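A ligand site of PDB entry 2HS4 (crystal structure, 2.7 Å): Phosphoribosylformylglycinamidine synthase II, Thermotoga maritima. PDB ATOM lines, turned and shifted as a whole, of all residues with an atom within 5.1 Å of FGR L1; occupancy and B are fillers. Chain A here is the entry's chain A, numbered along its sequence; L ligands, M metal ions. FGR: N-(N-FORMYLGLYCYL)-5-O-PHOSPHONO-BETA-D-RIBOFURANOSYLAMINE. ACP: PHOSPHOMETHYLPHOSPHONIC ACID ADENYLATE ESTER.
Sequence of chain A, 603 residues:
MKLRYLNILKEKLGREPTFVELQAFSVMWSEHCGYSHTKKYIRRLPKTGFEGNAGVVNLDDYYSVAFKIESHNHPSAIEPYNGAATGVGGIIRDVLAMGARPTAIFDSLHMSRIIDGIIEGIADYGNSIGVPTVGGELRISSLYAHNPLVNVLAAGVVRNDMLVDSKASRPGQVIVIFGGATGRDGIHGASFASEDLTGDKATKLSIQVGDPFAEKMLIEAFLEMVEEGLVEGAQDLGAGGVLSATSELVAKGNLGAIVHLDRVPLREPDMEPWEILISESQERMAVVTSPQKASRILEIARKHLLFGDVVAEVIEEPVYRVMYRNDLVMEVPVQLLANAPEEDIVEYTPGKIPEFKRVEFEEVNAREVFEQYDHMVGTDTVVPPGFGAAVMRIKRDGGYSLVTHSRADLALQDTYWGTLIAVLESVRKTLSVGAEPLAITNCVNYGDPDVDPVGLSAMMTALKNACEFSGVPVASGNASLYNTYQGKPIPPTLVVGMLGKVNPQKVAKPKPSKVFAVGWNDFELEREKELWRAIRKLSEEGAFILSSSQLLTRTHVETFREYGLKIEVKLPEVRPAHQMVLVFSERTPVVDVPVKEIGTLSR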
ATOM      1  N   HIS A  32      14.808 -10.241 -25.637  1.00  0.00           N
ATOM      2  CA  HIS A  32      13.436 -10.283 -25.147  1.00  0.00           C
ATOM      3  C   HIS A  32      13.128  -9.214 -24.099  1.00  0.00           C
ATOM      4  O   HIS A  32      12.044  -8.634 -24.118  1.00  0.00           O
ATOM      5  CB  HIS A  32      13.107 -11.661 -24.557  1.00  0.00           C
ATOM      6  CG  HIS A  32      11.717 -11.734 -23.989  1.00  0.00           C
ATOM      7  ND1 HIS A  32      10.592 -11.846 -24.782  1.00  0.00           N
ATOM      8  CD2 HIS A  32      11.260 -11.621 -22.714  1.00  0.00           C
ATOM      9  CE1 HIS A  32       9.512 -11.785 -24.028  1.00  0.00           C
ATOM     10  NE2 HIS A  32       9.889 -11.653 -22.775  1.00  0.00           N
ATOM     11  N   GLU A  70       0.958  -9.543 -27.047  1.00  0.00           N
ATOM     12  CA  GLU A  70       2.260 -10.129 -26.774  1.00  0.00           C
ATOM     13  C   GLU A  70       2.286 -11.424 -27.549  1.00  0.00           C
ATOM     14  O   GLU A  70       1.325 -11.746 -28.273  1.00  0.00           O
ATOM     15  CB  GLU A  70       2.459 -10.404 -25.279  1.00  0.00           C
ATOM     16  CG  GLU A  70       2.845  -9.162 -24.452  1.00  0.00           C
ATOM     17  CD  GLU A  70       3.246  -9.506 -23.010  1.00  0.00           C
ATOM     18  OE1 GLU A  70       2.474 -10.205 -22.320  1.00  0.00           O
ATOM     19  OE2 GLU A  70       4.325  -9.056 -22.562  1.00  0.00           O
ATOM     20  N   SER A  71       3.368 -12.177 -27.421  1.00  0.00           N
ATOM     21  CA  SER A  71       3.487 -13.427 -28.122  1.00  0.00           C
ATOM     22  C   SER A  71       4.225 -14.438 -27.272  1.00  0.00           C
ATOM     23  O   SER A  71       4.858 -14.083 -26.282  1.00  0.00           O
ATOM     24  CB  SER A  71       4.221 -13.214 -29.435  1.00  0.00           C
ATOM     25  OG  SER A  71       5.541 -12.784 -29.178  1.00  0.00           O
ATOM     26  N   HIS A  72       4.130 -15.694 -27.666  1.00  0.00           N
ATOM     27  CA  HIS A  72       4.788 -16.795 -26.989  1.00  0.00           C
ATOM     28  C   HIS A  72       5.214 -17.771 -28.096  1.00  0.00           C
ATOM     29  O   HIS A  72       4.760 -18.923 -28.142  1.00  0.00           O
ATOM     30  CB  HIS A  72       3.825 -17.498 -26.047  1.00  0.00           C
ATOM     31  CG  HIS A  72       4.297 -17.550 -24.618  1.00  0.00           C
ATOM     32  ND1 HIS A  72       4.307 -18.716 -23.878  1.00  0.00           N
ATOM     33  CD2 HIS A  72       4.705 -16.561 -23.784  1.00  0.00           C
ATOM     34  CE1 HIS A  72       4.688 -18.445 -22.643  1.00  0.00           C
ATOM     35  NE2 HIS A  72       4.936 -17.144 -22.563  1.00  0.00           N
ATOM     36  N   ASN A  73       6.084 -17.285 -28.959  1.00  0.00           N
ATOM     37  CA  ASN A  73       6.569 -18.064 -30.080  1.00  0.00           C
ATOM     38  C   ASN A  73       7.548 -19.171 -29.737  1.00  0.00           C
ATOM     39  O   ASN A  73       7.233 -20.347 -29.943  1.00  0.00           O
ATOM     40  CB  ASN A  73       7.176 -17.122 -31.123  1.00  0.00           C
ATOM     41  CG  ASN A  73       6.171 -16.112 -31.640  1.00  0.00           C
ATOM     42  OD1 ASN A  73       4.961 -16.364 -31.622  1.00  0.00           O
ATOM     43  ND2 ASN A  73       6.658 -14.974 -32.110  1.00  0.00           N
ATOM     44  N   HIS A  74       8.724 -18.822 -29.214  1.00  0.00           N
ATOM     45  CA  HIS A  74       9.718 -19.853 -28.902  1.00  0.00           C
ATOM     46  C   HIS A  74       9.160 -20.949 -27.981  1.00  0.00           C
ATOM     47  O   HIS A  74       9.378 -22.143 -28.223  1.00  0.00           O
ATOM     48  CB  HIS A  74      10.990 -19.225 -28.294  1.00  0.00           C
ATOM     49  CG  HIS A  74      11.770 -18.398 -29.267  1.00  0.00           C
ATOM     50  ND1 HIS A  74      11.432 -17.093 -29.573  1.00  0.00           N
ATOM     51  CD2 HIS A  74      12.847 -18.692 -30.031  1.00  0.00           C
ATOM     52  CE1 HIS A  74      12.270 -16.623 -30.483  1.00  0.00           C
ATOM     53  NE2 HIS A  74      13.133 -17.577 -30.780  1.00  0.00           N
ATOM     54  N   PRO A  75       8.416 -20.573 -26.933  1.00  0.00           N
ATOM     55  CA  PRO A  75       7.861 -21.595 -26.038  1.00  0.00           C
ATOM     56  C   PRO A  75       6.928 -22.567 -26.759  1.00  0.00           C
ATOM     57  O   PRO A  75       6.959 -23.776 -26.516  1.00  0.00           O
ATOM     58  CB  PRO A  75       7.104 -20.790 -24.993  1.00  0.00           C
ATOM     59  CG  PRO A  75       7.741 -19.446 -25.038  1.00  0.00           C
ATOM     60  CD  PRO A  75       8.027 -19.221 -26.490  1.00  0.00           C
ATOM     61  N   THR A  86       0.095 -20.431 -21.325  1.00  0.00           N
ATOM     62  CA  THR A  86       0.906 -19.487 -20.592  1.00  0.00           C
ATOM     63  C   THR A  86       0.963 -18.124 -21.293  1.00  0.00           C
ATOM     64  O   THR A  86       1.003 -17.088 -20.633  1.00  0.00           O
ATOM     65  CB  THR A  86       2.316 -20.039 -20.402  1.00  0.00           C
ATOM     66  OG1 THR A  86       2.224 -21.264 -19.668  1.00  0.00           O
ATOM     67  CG2 THR A  86       3.169 -19.074 -19.635  1.00  0.00           C
ATOM     68  N   GLY A  90       0.011 -14.766 -19.392  1.00  0.00           N
ATOM     69  CA  GLY A  90       0.829 -13.578 -19.325  1.00  0.00           C
ATOM     70  C   GLY A  90       0.232 -12.282 -19.860  1.00  0.00           C
ATOM     71  O   GLY A  90       0.361 -11.244 -19.228  1.00  0.00           O
ATOM     72  N   ARG A  93      -2.306 -10.891 -17.486  1.00  0.00           N
ATOM     73  CA  ARG A  93      -1.700 -10.239 -16.329  1.00  0.00           C
ATOM     74  C   ARG A  93      -1.276  -8.805 -16.684  1.00  0.00           C
ATOM     75  O   ARG A  93      -1.298  -7.925 -15.828  1.00  0.00           O
ATOM     76  CB  ARG A  93      -0.473 -11.020 -15.831  1.00  0.00           C
ATOM     77  CG  ARG A  93      -0.770 -12.188 -14.877  1.00  0.00           C
ATOM     78  CD  ARG A  93       0.524 -12.772 -14.317  1.00  0.00           C
ATOM     79  NE  ARG A  93       1.377 -13.344 -15.369  1.00  0.00           N
ATOM     80  CZ  ARG A  93       1.182 -14.541 -15.917  1.00  0.00           C
ATOM     81  NH1 ARG A  93       0.176 -15.301 -15.504  1.00  0.00           N
ATOM     82  NH2 ARG A  93       1.969 -14.973 -16.876  1.00  0.00           N
ATOM     83  N   GLY A 189      14.089 -18.413 -19.387  1.00  0.00           N
ATOM     84  CA  GLY A 189      13.188 -18.555 -20.514  1.00  0.00           C
ATOM     85  C   GLY A 189      13.173 -17.301 -21.373  1.00  0.00           C
ATOM     86  O   GLY A 189      12.689 -17.308 -22.508  1.00  0.00           O
ATOM     87  N   ALA A 190      13.710 -16.219 -20.818  1.00  0.00           N
ATOM     88  CA  ALA A 190      13.779 -14.946 -21.538  1.00  0.00           C
ATOM     89  C   ALA A 190      15.013 -14.951 -22.445  1.00  0.00           C
ATOM     90  O   ALA A 190      15.027 -14.311 -23.497  1.00  0.00           O
ATOM     91  CB  ALA A 190      13.846 -13.790 -20.540  1.00  0.00           C
ATOM     92  N   PHE A 192      16.096 -17.710 -23.606  1.00  0.00           N
ATOM     93  CA  PHE A 192      15.725 -18.763 -24.543  1.00  0.00           C
ATOM     94  C   PHE A 192      14.974 -18.160 -25.732  1.00  0.00           C
ATOM     95  O   PHE A 192      15.202 -18.543 -26.884  1.00  0.00           O
ATOM     96  CB  PHE A 192      14.854 -19.795 -23.805  1.00  0.00           C
ATOM     97  CG  PHE A 192      13.943 -20.576 -24.696  1.00  0.00           C
ATOM     98  CD1 PHE A 192      14.449 -21.389 -25.700  1.00  0.00           C
ATOM     99  CD2 PHE A 192      12.559 -20.489 -24.536  1.00  0.00           C
ATOM    100  CE1 PHE A 192      13.592 -22.120 -26.532  1.00  0.00           C
ATOM    101  CE2 PHE A 192      11.700 -21.203 -25.351  1.00  0.00           C
ATOM    102  CZ  PHE A 192      12.213 -22.023 -26.360  1.00  0.00           C
ATOM    103  N   ALA A 193      14.104 -17.201 -25.453  1.00  0.00           N
ATOM    104  CA  ALA A 193      13.300 -16.542 -26.489  1.00  0.00           C
ATOM    105  C   ALA A 193      14.086 -15.511 -27.303  1.00  0.00           C
ATOM    106  O   ALA A 193      13.517 -14.826 -28.164  1.00  0.00           O
ATOM    107  CB  ALA A 193      12.071 -15.882 -25.846  1.00  0.00           C
ATOM    108  N   SER A 206      13.047 -24.266 -19.692  1.00  0.00           N
ATOM    109  CA  SER A 206      12.764 -22.862 -19.982  1.00  0.00           C
ATOM    110  C   SER A 206      11.269 -22.578 -20.168  1.00  0.00           C
ATOM    111  O   SER A 206      10.867 -21.417 -20.318  1.00  0.00           O
ATOM    112  CB  SER A 206      13.515 -22.423 -21.236  1.00  0.00           C
ATOM    113  OG  SER A 206      14.914 -22.536 -21.059  1.00  0.00           O
ATOM    114  N   GLN A 208       7.330 -22.253 -19.062  1.00  0.00           N
ATOM    115  CA  GLN A 208       6.540 -21.895 -17.885  1.00  0.00           C
ATOM    116  C   GLN A 208       5.356 -22.856 -17.792  1.00  0.00           C
ATOM    117  O   GLN A 208       4.844 -23.289 -18.813  1.00  0.00           O
ATOM    118  CB  GLN A 208       6.071 -20.440 -18.010  1.00  0.00           C
ATOM    119  CG  GLN A 208       7.202 -19.407 -17.923  1.00  0.00           C
ATOM    120  CD  GLN A 208       6.877 -18.062 -18.585  1.00  0.00           C
ATOM    121  OE1 GLN A 208       7.540 -17.057 -18.334  1.00  0.00           O
ATOM    122  NE2 GLN A 208       5.873 -18.071 -19.446  1.00  0.00           N
ATOM    123  N   LEU A 237       4.403 -10.397 -13.396  1.00  0.00           N
ATOM    124  CA  LEU A 237       5.634 -11.147 -13.490  1.00  0.00           C
ATOM    125  C   LEU A 237       5.536 -12.097 -14.687  1.00  0.00           C
ATOM    126  O   LEU A 237       4.474 -12.630 -15.008  1.00  0.00           O
ATOM    127  CB  LEU A 237       5.918 -11.927 -12.203  1.00  0.00           C
ATOM    128  CG  LEU A 237       6.785 -11.190 -11.170  1.00  0.00           C
ATOM    129  CD1 LEU A 237       5.934 -10.174 -10.441  1.00  0.00           C
ATOM    130  CD2 LEU A 237       7.383 -12.177 -10.184  1.00  0.00           C
ATOM    131  N   GLY A 238       6.669 -12.286 -15.354  1.00  0.00           N
ATOM    132  CA  GLY A 238       6.725 -13.165 -16.507  1.00  0.00           C
ATOM    133  C   GLY A 238       8.171 -13.494 -16.765  1.00  0.00           C
ATOM    134  O   GLY A 238       8.764 -14.331 -16.084  1.00  0.00           O
ATOM    135  N   ALA A 239       8.768 -12.815 -17.746  1.00  0.00           N
ATOM    136  CA  ALA A 239      10.161 -13.038 -18.063  1.00  0.00           C
ATOM    137  C   ALA A 239      11.037 -12.247 -17.086  1.00  0.00           C
ATOM    138  O   ALA A 239      10.889 -11.028 -16.947  1.00  0.00           O
ATOM    139  CB  ALA A 239      10.426 -12.596 -19.475  1.00  0.00           C
ATOM    140  N   GLU A 280      10.639 -17.833 -13.489  1.00  0.00           N
ATOM    141  CA  GLU A 280       9.542 -17.273 -14.256  1.00  0.00           C
ATOM    142  C   GLU A 280       8.191 -17.930 -14.057  1.00  0.00           C
ATOM    143  O   GLU A 280       7.392 -17.997 -14.981  1.00  0.00           O
ATOM    144  CB  GLU A 280       9.936 -17.232 -15.730  1.00  0.00           C
ATOM    145  CG  GLU A 280      11.124 -16.297 -15.957  1.00  0.00           C
ATOM    146  CD  GLU A 280      11.487 -16.084 -17.412  1.00  0.00           C
ATOM    147  OE1 GLU A 280      10.569 -16.060 -18.256  1.00  0.00           O
ATOM    148  OE2 GLU A 280      12.700 -15.932 -17.687  1.00  0.00           O
ATOM    149  N   GLN A 282       4.381 -18.665 -13.103  1.00  0.00           N
ATOM    150  CA  GLN A 282       3.136 -17.960 -13.423  1.00  0.00           C
ATOM    151  C   GLN A 282       2.245 -17.582 -12.241  1.00  0.00           C
ATOM    152  O   GLN A 282       2.511 -17.914 -11.098  1.00  0.00           O
ATOM    153  CB  GLN A 282       2.319 -18.813 -14.388  1.00  0.00           C
ATOM    154  CG  GLN A 282       3.127 -19.318 -15.570  1.00  0.00           C
ATOM    155  CD  GLN A 282       3.589 -18.191 -16.450  1.00  0.00           C
ATOM    156  OE1 GLN A 282       2.790 -17.576 -17.163  1.00  0.00           O
ATOM    157  NE2 GLN A 282       4.885 -17.900 -16.393  1.00  0.00           N
ATOM    158  N   ALA A 479       7.698  -7.115 -29.486  1.00  0.00           N
ATOM    159  CA  ALA A 479       8.628  -7.413 -30.560  1.00  0.00           C
ATOM    160  C   ALA A 479       9.345  -8.725 -30.287  1.00  0.00           C
ATOM    161  O   ALA A 479      10.200  -8.812 -29.411  1.00  0.00           O
ATOM    162  CB  ALA A 479       9.626  -6.303 -30.742  1.00  0.00           C
ATOM    163  N   SER A 480       8.982  -9.746 -31.060  1.00  0.00           N
ATOM    164  CA  SER A 480       9.590 -11.057 -30.942  1.00  0.00           C
ATOM    165  C   SER A 480      10.604 -11.234 -32.074  1.00  0.00           C
ATOM    166  O   SER A 480      10.219 -11.288 -33.244  1.00  0.00           O
ATOM    167  CB  SER A 480       8.531 -12.149 -31.022  1.00  0.00           C
ATOM    168  OG  SER A 480       9.142 -13.427 -30.964  1.00  0.00           O
ATOM    169  N   LEU A 481      11.887 -11.302 -31.731  1.00  0.00           N
ATOM    170  CA  LEU A 481      12.914 -11.467 -32.730  1.00  0.00           C
ATOM    171  C   LEU A 481      13.595 -12.824 -32.601  1.00  0.00           C
ATOM    172  O   LEU A 481      13.348 -13.551 -31.642  1.00  0.00           O
ATOM    173  CB  LEU A 481      13.971 -10.357 -32.610  1.00  0.00           C
ATOM    174  CG  LEU A 481      13.468  -8.914 -32.747  1.00  0.00           C
ATOM    175  CD1 LEU A 481      14.653  -8.003 -32.968  1.00  0.00           C
ATOM    176  CD2 LEU A 481      12.487  -8.795 -33.909  1.00  0.00           C
ATOM    177  N   ASN A 483      13.225 -15.509 -34.525  1.00  0.00           N
ATOM    178  CA  ASN A 483      12.299 -16.606 -34.755  1.00  0.00           C
ATOM    179  C   ASN A 483      12.866 -17.305 -35.990  1.00  0.00           C
ATOM    180  O   ASN A 483      12.421 -17.070 -37.117  1.00  0.00           O
ATOM    181  CB  ASN A 483      10.879 -16.077 -35.016  1.00  0.00           C
ATOM    182  CG  ASN A 483      10.217 -15.519 -33.758  1.00  0.00           C
ATOM    183  OD1 ASN A 483       9.849 -16.264 -32.841  1.00  0.00           O
ATOM    184  ND2 ASN A 483      10.068 -14.188 -33.699  1.00  0.00           N
HETATM  185  C1  FGR L   1       8.930 -16.896 -22.915  1.00  0.00           C
HETATM  186  O6  FGR L   1       9.817 -18.024 -23.172  1.00  0.00           O
HETATM  187  C2  FGR L   1       9.015 -16.211 -21.553  1.00  0.00           C
HETATM  188  O8  FGR L   1      10.303 -16.315 -20.940  1.00  0.00           O
HETATM  189  C3  FGR L   1       8.617 -14.804 -21.859  1.00  0.00           C
HETATM  190  O4  FGR L   1       8.690 -14.618 -23.262  1.00  0.00           O
HETATM  191  C5  FGR L   1       9.172 -15.805 -23.935  1.00  0.00           C
HETATM  192  C10 FGR L   1       8.493 -15.863 -25.305  1.00  0.00           C
HETATM  193  O12 FGR L   1       8.884 -14.779 -26.166  1.00  0.00           O
HETATM  194  N19 FGR L   1       7.276 -14.518 -21.354  1.00  0.00           N
HETATM  195  C21 FGR L   1       6.737 -13.294 -21.155  1.00  0.00           C
HETATM  196  O22 FGR L   1       7.347 -12.281 -21.398  1.00  0.00           O
HETATM  197  C23 FGR L   1       5.341 -13.193 -20.601  1.00  0.00           C
HETATM  198  N24 FGR L   1       4.753 -14.536 -20.339  1.00  0.00           N
HETATM  199  P15 FGR L   1       8.656 -14.855 -27.774  1.00  0.00           P
HETATM  200  O16 FGR L   1       7.133 -14.889 -27.984  1.00  0.00           O
HETATM  201  O17 FGR L   1       9.348 -16.052 -28.350  1.00  0.00           O
HETATM  202  O18 FGR L   1       9.252 -13.538 -28.295  1.00  0.00           O
HETATM  203  C19 FGR L   1       4.805 -14.515 -18.975  1.00  0.00           C
HETATM  204  O20 FGR L   1       4.402 -15.479 -18.390  1.00  0.00           O
HETATM  205  PG  ACP L   2       7.764  -8.820 -19.573  1.00  0.00           P
HETATM  206  O1G ACP L   2       9.113  -8.723 -20.274  1.00  0.00           O
HETATM  207  O2G ACP L   2       6.833  -9.669 -20.362  1.00  0.00           O
HETATM  208  O3G ACP L   2       7.909  -9.276 -18.119  1.00  0.00           O
HETATM  209  PB  ACP L   2       6.781  -6.345 -20.519  1.00  0.00           P
HETATM  210  O1B ACP L   2       6.201  -5.098 -19.955  1.00  0.00           O
HETATM  211  O2B ACP L   2       5.905  -6.918 -21.557  1.00  0.00           O
HETATM  212  C3B ACP L   2       7.083  -7.270 -19.215  1.00  0.00           C
HETATM  213  PA  ACP L   2       8.692  -5.680 -22.863  1.00  0.00           P
HETATM  214  O1A ACP L   2       8.397  -6.954 -23.627  1.00  0.00           O
HETATM  215  O2A ACP L   2      10.153  -5.354 -22.767  1.00  0.00           O
HETATM  216  O3A ACP L   2       8.080  -5.786 -21.381  1.00  0.00           O
HETATM  217  O5' ACP L   2       7.683  -4.641 -23.574  1.00  0.00           O
HETATM  218  C5' ACP L   2       7.762  -3.296 -23.057  1.00  0.00           C
HETATM  219  C4' ACP L   2       6.962  -2.017 -23.472  1.00  0.00           C
HETATM  220  O4' ACP L   2       7.462  -1.468 -24.663  1.00  0.00           O
HETATM  221  C3' ACP L   2       5.614  -2.557 -23.761  1.00  0.00           C
HETATM  222  O3' ACP L   2       4.854  -2.628 -22.576  1.00  0.00           O
HETATM  223  C2' ACP L   2       5.081  -1.634 -24.873  1.00  0.00           C
HETATM  224  O2' ACP L   2       4.286  -0.601 -24.345  1.00  0.00           O
HETATM  225  C1' ACP L   2       6.348  -1.217 -25.536  1.00  0.00           C
HETATM  226  N9  ACP L   2       6.615  -1.881 -26.877  1.00  0.00           N
HETATM  227  C8  ACP L   2       7.329  -2.975 -27.207  1.00  0.00           C
HETATM  228  N7  ACP L   2       7.343  -3.294 -28.506  1.00  0.00           N
HETATM  229  C5  ACP L   2       6.590  -2.325 -29.044  1.00  0.00           C
HETATM  230  C6  ACP L   2       6.126  -1.987 -30.392  1.00  0.00           C
HETATM  231  N6  ACP L   2       6.473  -2.752 -31.470  1.00  0.00           N
HETATM  232  N1  ACP L   2       5.321  -0.874 -30.628  1.00  0.00           N
HETATM  233  C2  ACP L   2       4.932  -0.075 -29.566  1.00  0.00           C
HETATM  234  N3  ACP L   2       5.309  -0.305 -28.262  1.00  0.00           N
HETATM  235  C4  ACP L   2       6.120  -1.426 -28.053  1.00  0.00           C
HETATM  236 MG    MG M   1       6.664  -9.298 -24.048  1.00  0.00          MG
HETATM  237 MG    MG M   2       4.230  -8.919 -18.883  1.00  0.00          MG
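Merely in contact with FGR L1: Pro 75 (3.1 Å), Ala 193 (3.4 Å), Gly 238 (3.4 Å), Ala 239 (3.6 Å), Phe 192 (3.9 Å) and Thr 86 (3.999 Å). Hydrophobic or aromatic side chains within 4 Å of FGR L1: His 32, His 72, His 74, Pro 75, Phe 192, Ala 193 and Ala 239.
O17 of FGR L1 is in hydrogen-bond range of N of His 74 (3.0 Å). An oxygen (O17) of FGR L1 lies within hydrogen-bond range of a ring nitrogen (ND1) of His 74, at 2.6 Å. OG of Ser 480 sits at hydrogen-bond distance from O18 of FGR L1, at 2.7 Å. The side-chain carboxylate of Glu 280 sits at hydrogen-bond distance from an oxygen (O8) of FGR L1 (2.7 Å). The backbone NH (N) of Asn 73 lies within hydrogen-bond range of an oxygen (O16) of FGR L1, at 2.8 Å. An oxygen (O16) of FGR L1 sits close to the backbone carbonyl oxygen of Ser 71, at 3.0 Å. OG of Ser 71 is in hydrogen-bond range of O16 of FGR L1 (2.9 Å). NH2 of Arg 93 lies within hydrogen-bond range of O20 of FGR L1. An oxygen (O20) of FGR L1 lies close to the side-chain amide oxygen of Gln 282, at 2.9 Å. A ring nitrogen (NE2) of His 32 lies within hydrogen-bond range of an oxygen (O22) of FGR L1 (3.0 Å). O of Gly 189 lies within hydrogen-bond range of O8 of FGR L1, at 3.0 Å. The backbone NH (N) of His 72 lies within hydrogen-bond range of an oxygen (O16) of FGR L1 (3.1 Å). A ring nitrogen (NE2) of His 72 lies within hydrogen-bond range of a nitrogen (N24) of FGR L1, 3.4 Å away. NE2 of Gln 208 is in hydrogen-bond range of O20 of FGR L1, at 3.2 Å. N of Ala 190 lies within hydrogen-bond range of O8 of FGR L1 (3.4 Å). The side-chain carboxylate (OE2) of Glu 70 sits close to an oxygen (O2B) of ACP L2, 2.8 Å away.
The side-chain amide nitrogen (ND2) of Asn 73 is in hydrogen-bond range of the side-chain hydroxyl (OG) of Ser 480, 3.1 Å away. The backbone carbonyl oxygen of Ser 480 sits at hydrogen-bond distance from the side-chain amide nitrogen of Asn 483 (2.9 Å). The backbone carbonyl oxygen of Glu 280 sits at hydrogen-bond distance from the side-chain amide nitrogen of Gln 282 (2.9 Å). OE2 of Glu 280 is in hydrogen-bond range of N of Gly 189 (3.3 Å). The backbone NH (N) of Ala 190 is in hydrogen-bond range of the side-chain carboxylate (OE2) of Glu 280 (3.3 Å). NH2 of Arg 93 lies within hydrogen-bond range of OE1 of Gln 282, at 2.7 Å. NE of Arg 93 sits at hydrogen-bond distance from O of Leu 237 (3.2 Å). A ring nitrogen (NE2) of His 72 is in hydrogen-bond range of the side-chain amide nitrogen (NE2) of Gln 208.
An oxygen (O2G) of ACP L2 lies close to an oxygen (O22) of FGR L1.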
